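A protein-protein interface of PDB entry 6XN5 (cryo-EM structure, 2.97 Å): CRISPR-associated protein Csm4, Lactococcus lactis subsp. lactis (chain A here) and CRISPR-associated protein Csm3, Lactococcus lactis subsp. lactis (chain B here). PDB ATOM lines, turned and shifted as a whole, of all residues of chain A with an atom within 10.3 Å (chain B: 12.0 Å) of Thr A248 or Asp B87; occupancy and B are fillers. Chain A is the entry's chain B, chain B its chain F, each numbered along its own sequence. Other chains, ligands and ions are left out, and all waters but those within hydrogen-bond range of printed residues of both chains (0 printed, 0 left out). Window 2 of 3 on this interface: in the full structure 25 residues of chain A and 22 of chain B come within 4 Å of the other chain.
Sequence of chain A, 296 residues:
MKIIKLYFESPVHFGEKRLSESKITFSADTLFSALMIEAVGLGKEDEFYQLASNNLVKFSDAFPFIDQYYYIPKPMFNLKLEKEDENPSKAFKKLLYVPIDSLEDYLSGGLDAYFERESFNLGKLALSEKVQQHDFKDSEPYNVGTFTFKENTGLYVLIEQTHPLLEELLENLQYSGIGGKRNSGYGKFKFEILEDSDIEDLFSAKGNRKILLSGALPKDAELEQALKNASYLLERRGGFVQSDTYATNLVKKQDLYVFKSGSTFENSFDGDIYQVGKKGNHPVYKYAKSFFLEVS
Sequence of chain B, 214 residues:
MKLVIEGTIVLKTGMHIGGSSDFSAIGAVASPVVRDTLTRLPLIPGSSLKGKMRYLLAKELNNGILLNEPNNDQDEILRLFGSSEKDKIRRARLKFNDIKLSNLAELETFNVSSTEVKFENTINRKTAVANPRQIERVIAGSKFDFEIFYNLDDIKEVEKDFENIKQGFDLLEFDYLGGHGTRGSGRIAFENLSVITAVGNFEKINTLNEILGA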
ATOM      1  N   VAL A 241      22.079  22.688 -18.518  1.00  0.00           N
ATOM      2  CA  VAL A 241      21.703  22.178 -19.829  1.00  0.00           C
ATOM      3  C   VAL A 241      21.805  20.661 -19.818  1.00  0.00           C
ATOM      4  O   VAL A 241      22.821  20.099 -19.397  1.00  0.00           O
ATOM      5  CB  VAL A 241      22.591  22.790 -20.917  1.00  0.00           C
ATOM      6  CG1 VAL A 241      22.141  22.345 -22.273  1.00  0.00           C
ATOM      7  CG2 VAL A 241      22.558  24.288 -20.820  1.00  0.00           C
ATOM      8  N   SER A 243      21.976  17.716 -22.218  1.00  0.00           N
ATOM      9  CA  SER A 243      22.230  17.171 -23.547  1.00  0.00           C
ATOM     10  C   SER A 243      23.567  16.447 -23.507  1.00  0.00           C
ATOM     11  O   SER A 243      24.139  16.221 -22.437  1.00  0.00           O
ATOM     12  CB  SER A 243      22.242  18.261 -24.619  1.00  0.00           C
ATOM     13  OG  SER A 243      23.458  18.970 -24.572  1.00  0.00           O
ATOM     14  N   ASP A 244      24.071  16.081 -24.682  1.00  0.00           N
ATOM     15  CA  ASP A 244      25.420  15.564 -24.800  1.00  0.00           C
ATOM     16  C   ASP A 244      26.297  16.389 -25.718  1.00  0.00           C
ATOM     17  O   ASP A 244      27.523  16.312 -25.603  1.00  0.00           O
ATOM     18  CB  ASP A 244      25.423  14.128 -25.325  1.00  0.00           C
ATOM     19  CG  ASP A 244      24.861  13.150 -24.342  1.00  0.00           C
ATOM     20  OD1 ASP A 244      24.970  13.400 -23.125  1.00  0.00           O
ATOM     21  OD2 ASP A 244      24.364  12.099 -24.794  1.00  0.00           O
ATOM     22  N   THR A 245      25.719  17.164 -26.626  1.00  0.00           N
ATOM     23  CA  THR A 245      26.500  17.821 -27.660  1.00  0.00           C
ATOM     24  C   THR A 245      26.765  19.280 -27.321  1.00  0.00           C
ATOM     25  O   THR A 245      27.324  20.013 -28.132  1.00  0.00           O
ATOM     26  CB  THR A 245      25.809  17.705 -29.014  1.00  0.00           C
ATOM     27  OG1 THR A 245      24.484  18.239 -28.922  1.00  0.00           O
ATOM     28  CG2 THR A 245      25.731  16.251 -29.437  1.00  0.00           C
ATOM     29  N   TYR A 246      26.392  19.716 -26.127  1.00  0.00           N
ATOM     30  CA  TYR A 246      26.568  21.103 -25.718  1.00  0.00           C
ATOM     31  C   TYR A 246      27.822  21.196 -24.860  1.00  0.00           C
ATOM     32  O   TYR A 246      27.850  20.686 -23.736  1.00  0.00           O
ATOM     33  CB  TYR A 246      25.338  21.603 -24.965  1.00  0.00           C
ATOM     34  CG  TYR A 246      25.227  23.102 -24.834  1.00  0.00           C
ATOM     35  CD1 TYR A 246      25.924  23.789 -23.857  1.00  0.00           C
ATOM     36  CD2 TYR A 246      24.397  23.826 -25.668  1.00  0.00           C
ATOM     37  CE1 TYR A 246      25.821  25.148 -23.736  1.00  0.00           C
ATOM     38  CE2 TYR A 246      24.287  25.190 -25.550  1.00  0.00           C
ATOM     39  CZ  TYR A 246      25.005  25.840 -24.582  1.00  0.00           C
ATOM     40  OH  TYR A 246      24.908  27.199 -24.447  1.00  0.00           O
ATOM     41  N   ALA A 247      28.868  21.804 -25.414  1.00  0.00           N
ATOM     42  CA  ALA A 247      29.998  22.402 -24.706  1.00  0.00           C
ATOM     43  C   ALA A 247      30.852  21.439 -23.889  1.00  0.00           C
ATOM     44  O   ALA A 247      31.600  21.908 -23.029  1.00  0.00           O
ATOM     45  CB  ALA A 247      29.538  23.534 -23.782  1.00  0.00           C
ATOM     46  N   THR A 248      30.729  20.119 -24.092  1.00  0.00           N
ATOM     47  CA  THR A 248      31.594  19.023 -23.578  1.00  0.00           C
ATOM     48  C   THR A 248      31.858  19.061 -22.057  1.00  0.00           C
ATOM     49  O   THR A 248      32.733  18.346 -21.561  1.00  0.00           O
ATOM     50  CB  THR A 248      32.926  18.906 -24.358  1.00  0.00           C
ATOM     51  OG1 THR A 248      33.536  17.647 -24.056  1.00  0.00           O
ATOM     52  CG2 THR A 248      33.962  19.995 -24.041  1.00  0.00           C
ATOM     53  N   ASN A 249      31.075  19.821 -21.297  1.00  0.00           N
ATOM     54  CA  ASN A 249      31.032  19.763 -19.841  1.00  0.00           C
ATOM     55  C   ASN A 249      29.709  20.370 -19.403  1.00  0.00           C
ATOM     56  O   ASN A 249      29.041  21.055 -20.180  1.00  0.00           O
ATOM     57  CB  ASN A 249      32.226  20.477 -19.185  1.00  0.00           C
ATOM     58  CG  ASN A 249      32.144  21.993 -19.268  1.00  0.00           C
ATOM     59  OD1 ASN A 249      31.680  22.560 -20.255  1.00  0.00           O
ATOM     60  ND2 ASN A 249      32.624  22.659 -18.225  1.00  0.00           N
ATOM     61  N   LEU A 250      29.329  20.090 -18.162  1.00  0.00           N
ATOM     62  CA  LEU A 250      28.088  20.607 -17.600  1.00  0.00           C
ATOM     63  C   LEU A 250      28.146  22.122 -17.471  1.00  0.00           C
ATOM     64  O   LEU A 250      29.156  22.688 -17.057  1.00  0.00           O
ATOM     65  CB  LEU A 250      27.845  19.986 -16.232  1.00  0.00           C
ATOM     66  CG  LEU A 250      26.995  18.735 -16.053  1.00  0.00           C
ATOM     67  CD1 LEU A 250      27.528  17.566 -16.816  1.00  0.00           C
ATOM     68  CD2 LEU A 250      27.056  18.413 -14.595  1.00  0.00           C
ATOM     69  N   VAL A 251      27.048  22.783 -17.829  1.00  0.00           N
ATOM     70  CA  VAL A 251      27.030  24.240 -17.896  1.00  0.00           C
ATOM     71  C   VAL A 251      25.608  24.720 -17.622  1.00  0.00           C
ATOM     72  O   VAL A 251      24.632  24.063 -17.990  1.00  0.00           O
ATOM     73  CB  VAL A 251      27.592  24.725 -19.256  1.00  0.00           C
ATOM     74  CG1 VAL A 251      26.751  24.242 -20.393  1.00  0.00           C
ATOM     75  CG2 VAL A 251      27.755  26.234 -19.304  1.00  0.00           C
ATOM     76  N   LYS A 279      26.324  29.720 -26.355  1.00  0.00           N
ATOM     77  CA  LYS A 279      27.727  29.335 -26.501  1.00  0.00           C
ATOM     78  C   LYS A 279      27.874  27.814 -26.509  1.00  0.00           C
ATOM     79  O   LYS A 279      28.570  27.224 -25.689  1.00  0.00           O
ATOM     80  CB  LYS A 279      28.560  29.968 -25.393  1.00  0.00           C
ATOM     81  CG  LYS A 279      28.559  31.483 -25.415  1.00  0.00           C
ATOM     82  CD  LYS A 279      29.522  32.054 -24.397  1.00  0.00           C
ATOM     83  CE  LYS A 279      28.987  31.919 -22.989  1.00  0.00           C
ATOM     84  NZ  LYS A 279      27.790  32.773 -22.780  1.00  0.00           N
ATOM     85  N   GLY A 280      27.212  27.181 -27.467  1.00  0.00           N
ATOM     86  CA  GLY A 280      27.244  25.733 -27.568  1.00  0.00           C
ATOM     87  C   GLY A 280      26.981  25.314 -28.994  1.00  0.00           C
ATOM     88  O   GLY A 280      26.772  26.146 -29.880  1.00  0.00           O
ATOM     89  N   ASN A 281      26.998  23.998 -29.210  1.00  0.00           N
ATOM     90  CA  ASN A 281      26.860  23.486 -30.569  1.00  0.00           C
ATOM     91  C   ASN A 281      25.415  23.541 -31.049  1.00  0.00           C
ATOM     92  O   ASN A 281      25.159  23.571 -32.258  1.00  0.00           O
ATOM     93  CB  ASN A 281      27.405  22.065 -30.655  1.00  0.00           C
ATOM     94  CG  ASN A 281      28.847  21.975 -30.218  1.00  0.00           C
ATOM     95  OD1 ASN A 281      29.714  22.640 -30.778  1.00  0.00           O
ATOM     96  ND2 ASN A 281      29.114  21.152 -29.215  1.00  0.00           N
ATOM     97  N   HIS A 282      24.466  23.542 -30.130  1.00  0.00           N
ATOM     98  CA  HIS A 282      23.051  23.619 -30.442  1.00  0.00           C
ATOM     99  C   HIS A 282      22.386  24.643 -29.533  1.00  0.00           C
ATOM    100  O   HIS A 282      22.859  24.887 -28.419  1.00  0.00           O
ATOM    101  CB  HIS A 282      22.398  22.242 -30.271  1.00  0.00           C
ATOM    102  CG  HIS A 282      22.282  21.801 -28.850  1.00  0.00           C
ATOM    103  ND1 HIS A 282      21.202  22.118 -28.058  1.00  0.00           N
ATOM    104  CD2 HIS A 282      23.108  21.060 -28.080  1.00  0.00           C
ATOM    105  CE1 HIS A 282      21.371  21.596 -26.859  1.00  0.00           C
ATOM    106  NE2 HIS A 282      22.519  20.946 -26.846  1.00  0.00           N
ATOM    107  N   ASP B  73      35.480   3.679 -16.309  1.00  0.00           N
ATOM    108  CA  ASP B  73      34.951   2.437 -16.859  1.00  0.00           C
ATOM    109  C   ASP B  73      34.920   2.470 -18.379  1.00  0.00           C
ATOM    110  O   ASP B  73      35.004   3.535 -18.988  1.00  0.00           O
ATOM    111  CB  ASP B  73      33.551   2.168 -16.314  1.00  0.00           C
ATOM    112  CG  ASP B  73      33.569   1.635 -14.897  1.00  0.00           C
ATOM    113  OD1 ASP B  73      34.494   0.865 -14.561  1.00  0.00           O
ATOM    114  OD2 ASP B  73      32.657   1.988 -14.121  1.00  0.00           O
ATOM    115  N   ASP B  75      33.353   1.889 -22.271  1.00  0.00           N
ATOM    116  CA  ASP B  75      32.215   2.584 -22.862  1.00  0.00           C
ATOM    117  C   ASP B  75      30.944   1.747 -22.928  1.00  0.00           C
ATOM    118  O   ASP B  75      29.878   2.307 -23.194  1.00  0.00           O
ATOM    119  CB  ASP B  75      32.600   3.135 -24.242  1.00  0.00           C
ATOM    120  CG  ASP B  75      32.986   2.055 -25.246  1.00  0.00           C
ATOM    121  OD1 ASP B  75      33.020   0.857 -24.909  1.00  0.00           O
ATOM    122  OD2 ASP B  75      33.257   2.422 -26.409  1.00  0.00           O
ATOM    123  N   LEU B  78      29.295   2.858 -19.666  1.00  0.00           N
ATOM    124  CA  LEU B  78      28.888   4.254 -19.742  1.00  0.00           C
ATOM    125  C   LEU B  78      27.749   4.450 -20.730  1.00  0.00           C
ATOM    126  O   LEU B  78      26.868   5.282 -20.506  1.00  0.00           O
ATOM    127  CB  LEU B  78      30.076   5.128 -20.125  1.00  0.00           C
ATOM    128  CG  LEU B  78      31.303   4.981 -19.234  1.00  0.00           C
ATOM    129  CD1 LEU B  78      32.391   5.926 -19.682  1.00  0.00           C
ATOM    130  CD2 LEU B  78      30.960   5.193 -17.777  1.00  0.00           C
ATOM    131  N   ARG B  79      27.746   3.704 -21.832  1.00  0.00           N
ATOM    132  CA  ARG B  79      26.658   3.849 -22.789  1.00  0.00           C
ATOM    133  C   ARG B  79      25.398   3.148 -22.315  1.00  0.00           C
ATOM    134  O   ARG B  79      24.301   3.477 -22.775  1.00  0.00           O
ATOM    135  CB  ARG B  79      27.088   3.330 -24.158  1.00  0.00           C
ATOM    136  CG  ARG B  79      26.773   1.889 -24.446  1.00  0.00           C
ATOM    137  CD  ARG B  79      27.675   1.389 -25.547  1.00  0.00           C
ATOM    138  NE  ARG B  79      27.358   0.029 -25.952  1.00  0.00           N
ATOM    139  CZ  ARG B  79      28.150  -0.718 -26.707  1.00  0.00           C
ATOM    140  NH1 ARG B  79      29.302  -0.231 -27.134  1.00  0.00           N
ATOM    141  NH2 ARG B  79      27.790  -1.948 -27.031  1.00  0.00           N
ATOM    142  N   GLY B  82      24.949   5.638 -18.479  1.00  0.00           N
ATOM    143  CA  GLY B  82      25.145   7.068 -18.427  1.00  0.00           C
ATOM    144  C   GLY B  82      26.390   7.449 -17.659  1.00  0.00           C
ATOM    145  O   GLY B  82      26.851   6.754 -16.759  1.00  0.00           O
ATOM    146  N   SER B  83      26.947   8.594 -18.027  1.00  0.00           N
ATOM    147  CA  SER B  83      28.127   9.092 -17.342  1.00  0.00           C
ATOM    148  C   SER B  83      28.145  10.603 -17.448  1.00  0.00           C
ATOM    149  O   SER B  83      27.564  11.188 -18.363  1.00  0.00           O
ATOM    150  CB  SER B  83      29.414   8.517 -17.925  1.00  0.00           C
ATOM    151  OG  SER B  83      29.615   8.968 -19.250  1.00  0.00           O
ATOM    152  N   SER B  84      28.825  11.226 -16.495  1.00  0.00           N
ATOM    153  CA  SER B  84      29.031  12.667 -16.555  1.00  0.00           C
ATOM    154  C   SER B  84      30.403  12.946 -15.946  1.00  0.00           C
ATOM    155  O   SER B  84      30.538  13.104 -14.733  1.00  0.00           O
ATOM    156  CB  SER B  84      27.936  13.418 -15.828  1.00  0.00           C
ATOM    157  OG  SER B  84      28.152  13.375 -14.433  1.00  0.00           O
ATOM    158  N   GLU B  85      31.408  12.999 -16.808  1.00  0.00           N
ATOM    159  CA  GLU B  85      32.765  13.334 -16.427  1.00  0.00           C
ATOM    160  C   GLU B  85      33.098  14.693 -17.019  1.00  0.00           C
ATOM    161  O   GLU B  85      32.239  15.371 -17.586  1.00  0.00           O
ATOM    162  CB  GLU B  85      33.757  12.270 -16.904  1.00  0.00           C
ATOM    163  CG  GLU B  85      33.569  10.921 -16.243  1.00  0.00           C
ATOM    164  CD  GLU B  85      33.950  10.934 -14.778  1.00  0.00           C
ATOM    165  OE1 GLU B  85      34.921  11.635 -14.422  1.00  0.00           O
ATOM    166  OE2 GLU B  85      33.283  10.248 -13.980  1.00  0.00           O
ATOM    167  N   LYS B  86      34.361  15.092 -16.880  1.00  0.00           N
ATOM    168  CA  LYS B  86      34.792  16.378 -17.411  1.00  0.00           C
ATOM    169  C   LYS B  86      34.834  16.407 -18.931  1.00  0.00           C
ATOM    170  O   LYS B  86      34.857  17.499 -19.506  1.00  0.00           O
ATOM    171  CB  LYS B  86      36.165  16.747 -16.850  1.00  0.00           C
ATOM    172  CG  LYS B  86      36.336  16.500 -15.354  1.00  0.00           C
ATOM    173  CD  LYS B  86      35.302  17.261 -14.526  1.00  0.00           C
ATOM    174  CE  LYS B  86      35.701  18.720 -14.354  1.00  0.00           C
ATOM    175  NZ  LYS B  86      34.560  19.570 -13.920  1.00  0.00           N
ATOM    176  N   ASP B  87      34.857  15.253 -19.594  1.00  0.00           N
ATOM    177  CA  ASP B  87      34.789  15.225 -21.047  1.00  0.00           C
ATOM    178  C   ASP B  87      33.823  14.157 -21.535  1.00  0.00           C
ATOM    179  O   ASP B  87      33.339  14.223 -22.669  1.00  0.00           O
ATOM    180  CB  ASP B  87      36.174  15.000 -21.649  1.00  0.00           C
ATOM    181  CG  ASP B  87      36.352  15.707 -22.981  1.00  0.00           C
ATOM    182  OD1 ASP B  87      35.392  16.352 -23.447  1.00  0.00           O
ATOM    183  OD2 ASP B  87      37.449  15.609 -23.567  1.00  0.00           O
ATOM    184  N   LYS B  88      33.537  13.167 -20.693  1.00  0.00           N
ATOM    185  CA  LYS B  88      32.636  12.077 -21.060  1.00  0.00           C
ATOM    186  C   LYS B  88      31.267  12.358 -20.460  1.00  0.00           C
ATOM    187  O   LYS B  88      31.063  12.212 -19.255  1.00  0.00           O
ATOM    188  CB  LYS B  88      33.175  10.738 -20.575  1.00  0.00           C
ATOM    189  CG  LYS B  88      34.500  10.335 -21.180  1.00  0.00           C
ATOM    190  CD  LYS B  88      34.954   8.998 -20.630  1.00  0.00           C
ATOM    191  CE  LYS B  88      35.282   9.099 -19.155  1.00  0.00           C
ATOM    192  NZ  LYS B  88      36.431  10.010 -18.920  1.00  0.00           N
ATOM    193  N   ILE B  89      30.327  12.774 -21.303  1.00  0.00           N
ATOM    194  CA  ILE B  89      28.925  12.893 -20.931  1.00  0.00           C
ATOM    195  C   ILE B  89      28.117  12.075 -21.920  1.00  0.00           C
ATOM    196  O   ILE B  89      28.198  12.306 -23.132  1.00  0.00           O
ATOM    197  CB  ILE B  89      28.445  14.353 -20.932  1.00  0.00           C
ATOM    198  CG1 ILE B  89      29.210  15.176 -19.909  1.00  0.00           C
ATOM    199  CG2 ILE B  89      26.973  14.419 -20.629  1.00  0.00           C
ATOM    200  CD1 ILE B  89      29.008  16.640 -20.091  1.00  0.00           C
ATOM    201  N   ARG B  90      27.365  11.103 -21.414  1.00  0.00           N
ATOM    202  CA  ARG B  90      26.510  10.287 -22.258  1.00  0.00           C
ATOM    203  C   ARG B  90      25.141  10.188 -21.612  1.00  0.00           C
ATOM    204  O   ARG B  90      25.022  10.177 -20.386  1.00  0.00           O
ATOM    205  CB  ARG B  90      27.074   8.879 -22.475  1.00  0.00           C
ATOM    206  CG  ARG B  90      28.489   8.831 -23.001  1.00  0.00           C
ATOM    207  CD  ARG B  90      28.815   7.488 -23.579  1.00  0.00           C
ATOM    208  NE  ARG B  90      28.017   7.218 -24.765  1.00  0.00           N
ATOM    209  CZ  ARG B  90      28.324   6.297 -25.666  1.00  0.00           C
ATOM    210  NH1 ARG B  90      29.416   5.565 -25.513  1.00  0.00           N
ATOM    211  NH2 ARG B  90      27.544   6.109 -26.717  1.00  0.00           N
ATOM    212  N   ARG B  91      24.109  10.123 -22.442  1.00  0.00           N
ATOM    213  CA  ARG B  91      22.789   9.781 -21.948  1.00  0.00           C
ATOM    214  C   ARG B  91      22.712   8.288 -21.692  1.00  0.00           C
ATOM    215  O   ARG B  91      23.203   7.483 -22.487  1.00  0.00           O
ATOM    216  CB  ARG B  91      21.707  10.204 -22.935  1.00  0.00           C
ATOM    217  CG  ARG B  91      21.627  11.696 -23.133  1.00  0.00           C
ATOM    218  CD  ARG B  91      20.670  12.074 -24.246  1.00  0.00           C
ATOM    219  NE  ARG B  91      19.343  11.505 -24.049  1.00  0.00           N
ATOM    220  CZ  ARG B  91      18.542  11.132 -25.039  1.00  0.00           C
ATOM    221  NH1 ARG B  91      18.942  11.260 -26.295  1.00  0.00           N
ATOM    222  NH2 ARG B  91      17.347  10.629 -24.775  1.00  0.00           N
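The side-chain hydroxyl (OG) of Ser A243 lies close to the backbone NH (N) of Tyr A246 (3.4 Å). NE2 of His A282 sits at hydrogen-bond distance from OG of Ser A243. OD1 of Asn A249 sits close to O of Ala A247, 2.9 Å away. The backbone carbonyl oxygen (O) of Ser B83 sits at hydrogen-bond distance from the backbone NH (N) of Arg B90, at 3.1 Å.
Of chain A, only Thr A248 comes within 4 Å of Asp B87. Ala A247 touches none of the printed residues of chain B. No residue of chain A comes within 4 Å of Lys B88. Printed residues of chain B within 4 Å of Ser A243: Ile B89 (3.8 Å). Printed residues of chain A within 4 Å of Lys B86: Thr A248 (3.1 Å) and Asn A249 (3.99 Å). His A282 touches none of the printed residues of chain B. Ser B83 touches none of the printed residues of chain A. The nearest printed residue of chain B that does not touch Leu A250 is Ser B84 (4.3 Å).
Hydrophobic or aromatic side chains of chain A that line the printed part of chain B: Leu A250. Hydrophobic or aromatic side chains of chain B that line the printed part of chain A: Ile B89.
Ser A243 touches Ile B89 (O to CG2, 3.8 Å). OD1 of Asp A244 touches C of Arg B90, 3.6 Å away. Asn A249 touches Lys B86 (CB to O, 3.99 Å). CA of Asn A249 touches CD1 of Ile B89 (3.7 Å). Leu A250 touches Ile B89.
The side-chain carboxylate (OD1) of Asp A244 lies close to the backbone carbonyl oxygen (O) of Ile B89. O of Thr A248 lies close to O of Lys B86 (3.1 Å). OG1 of Thr A248 lies close to OD1 of Asp B87 (2.3 Å). OD2 of Asp A244 lies within hydrogen-bond range of N of Arg B91, 3.1 Å away.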
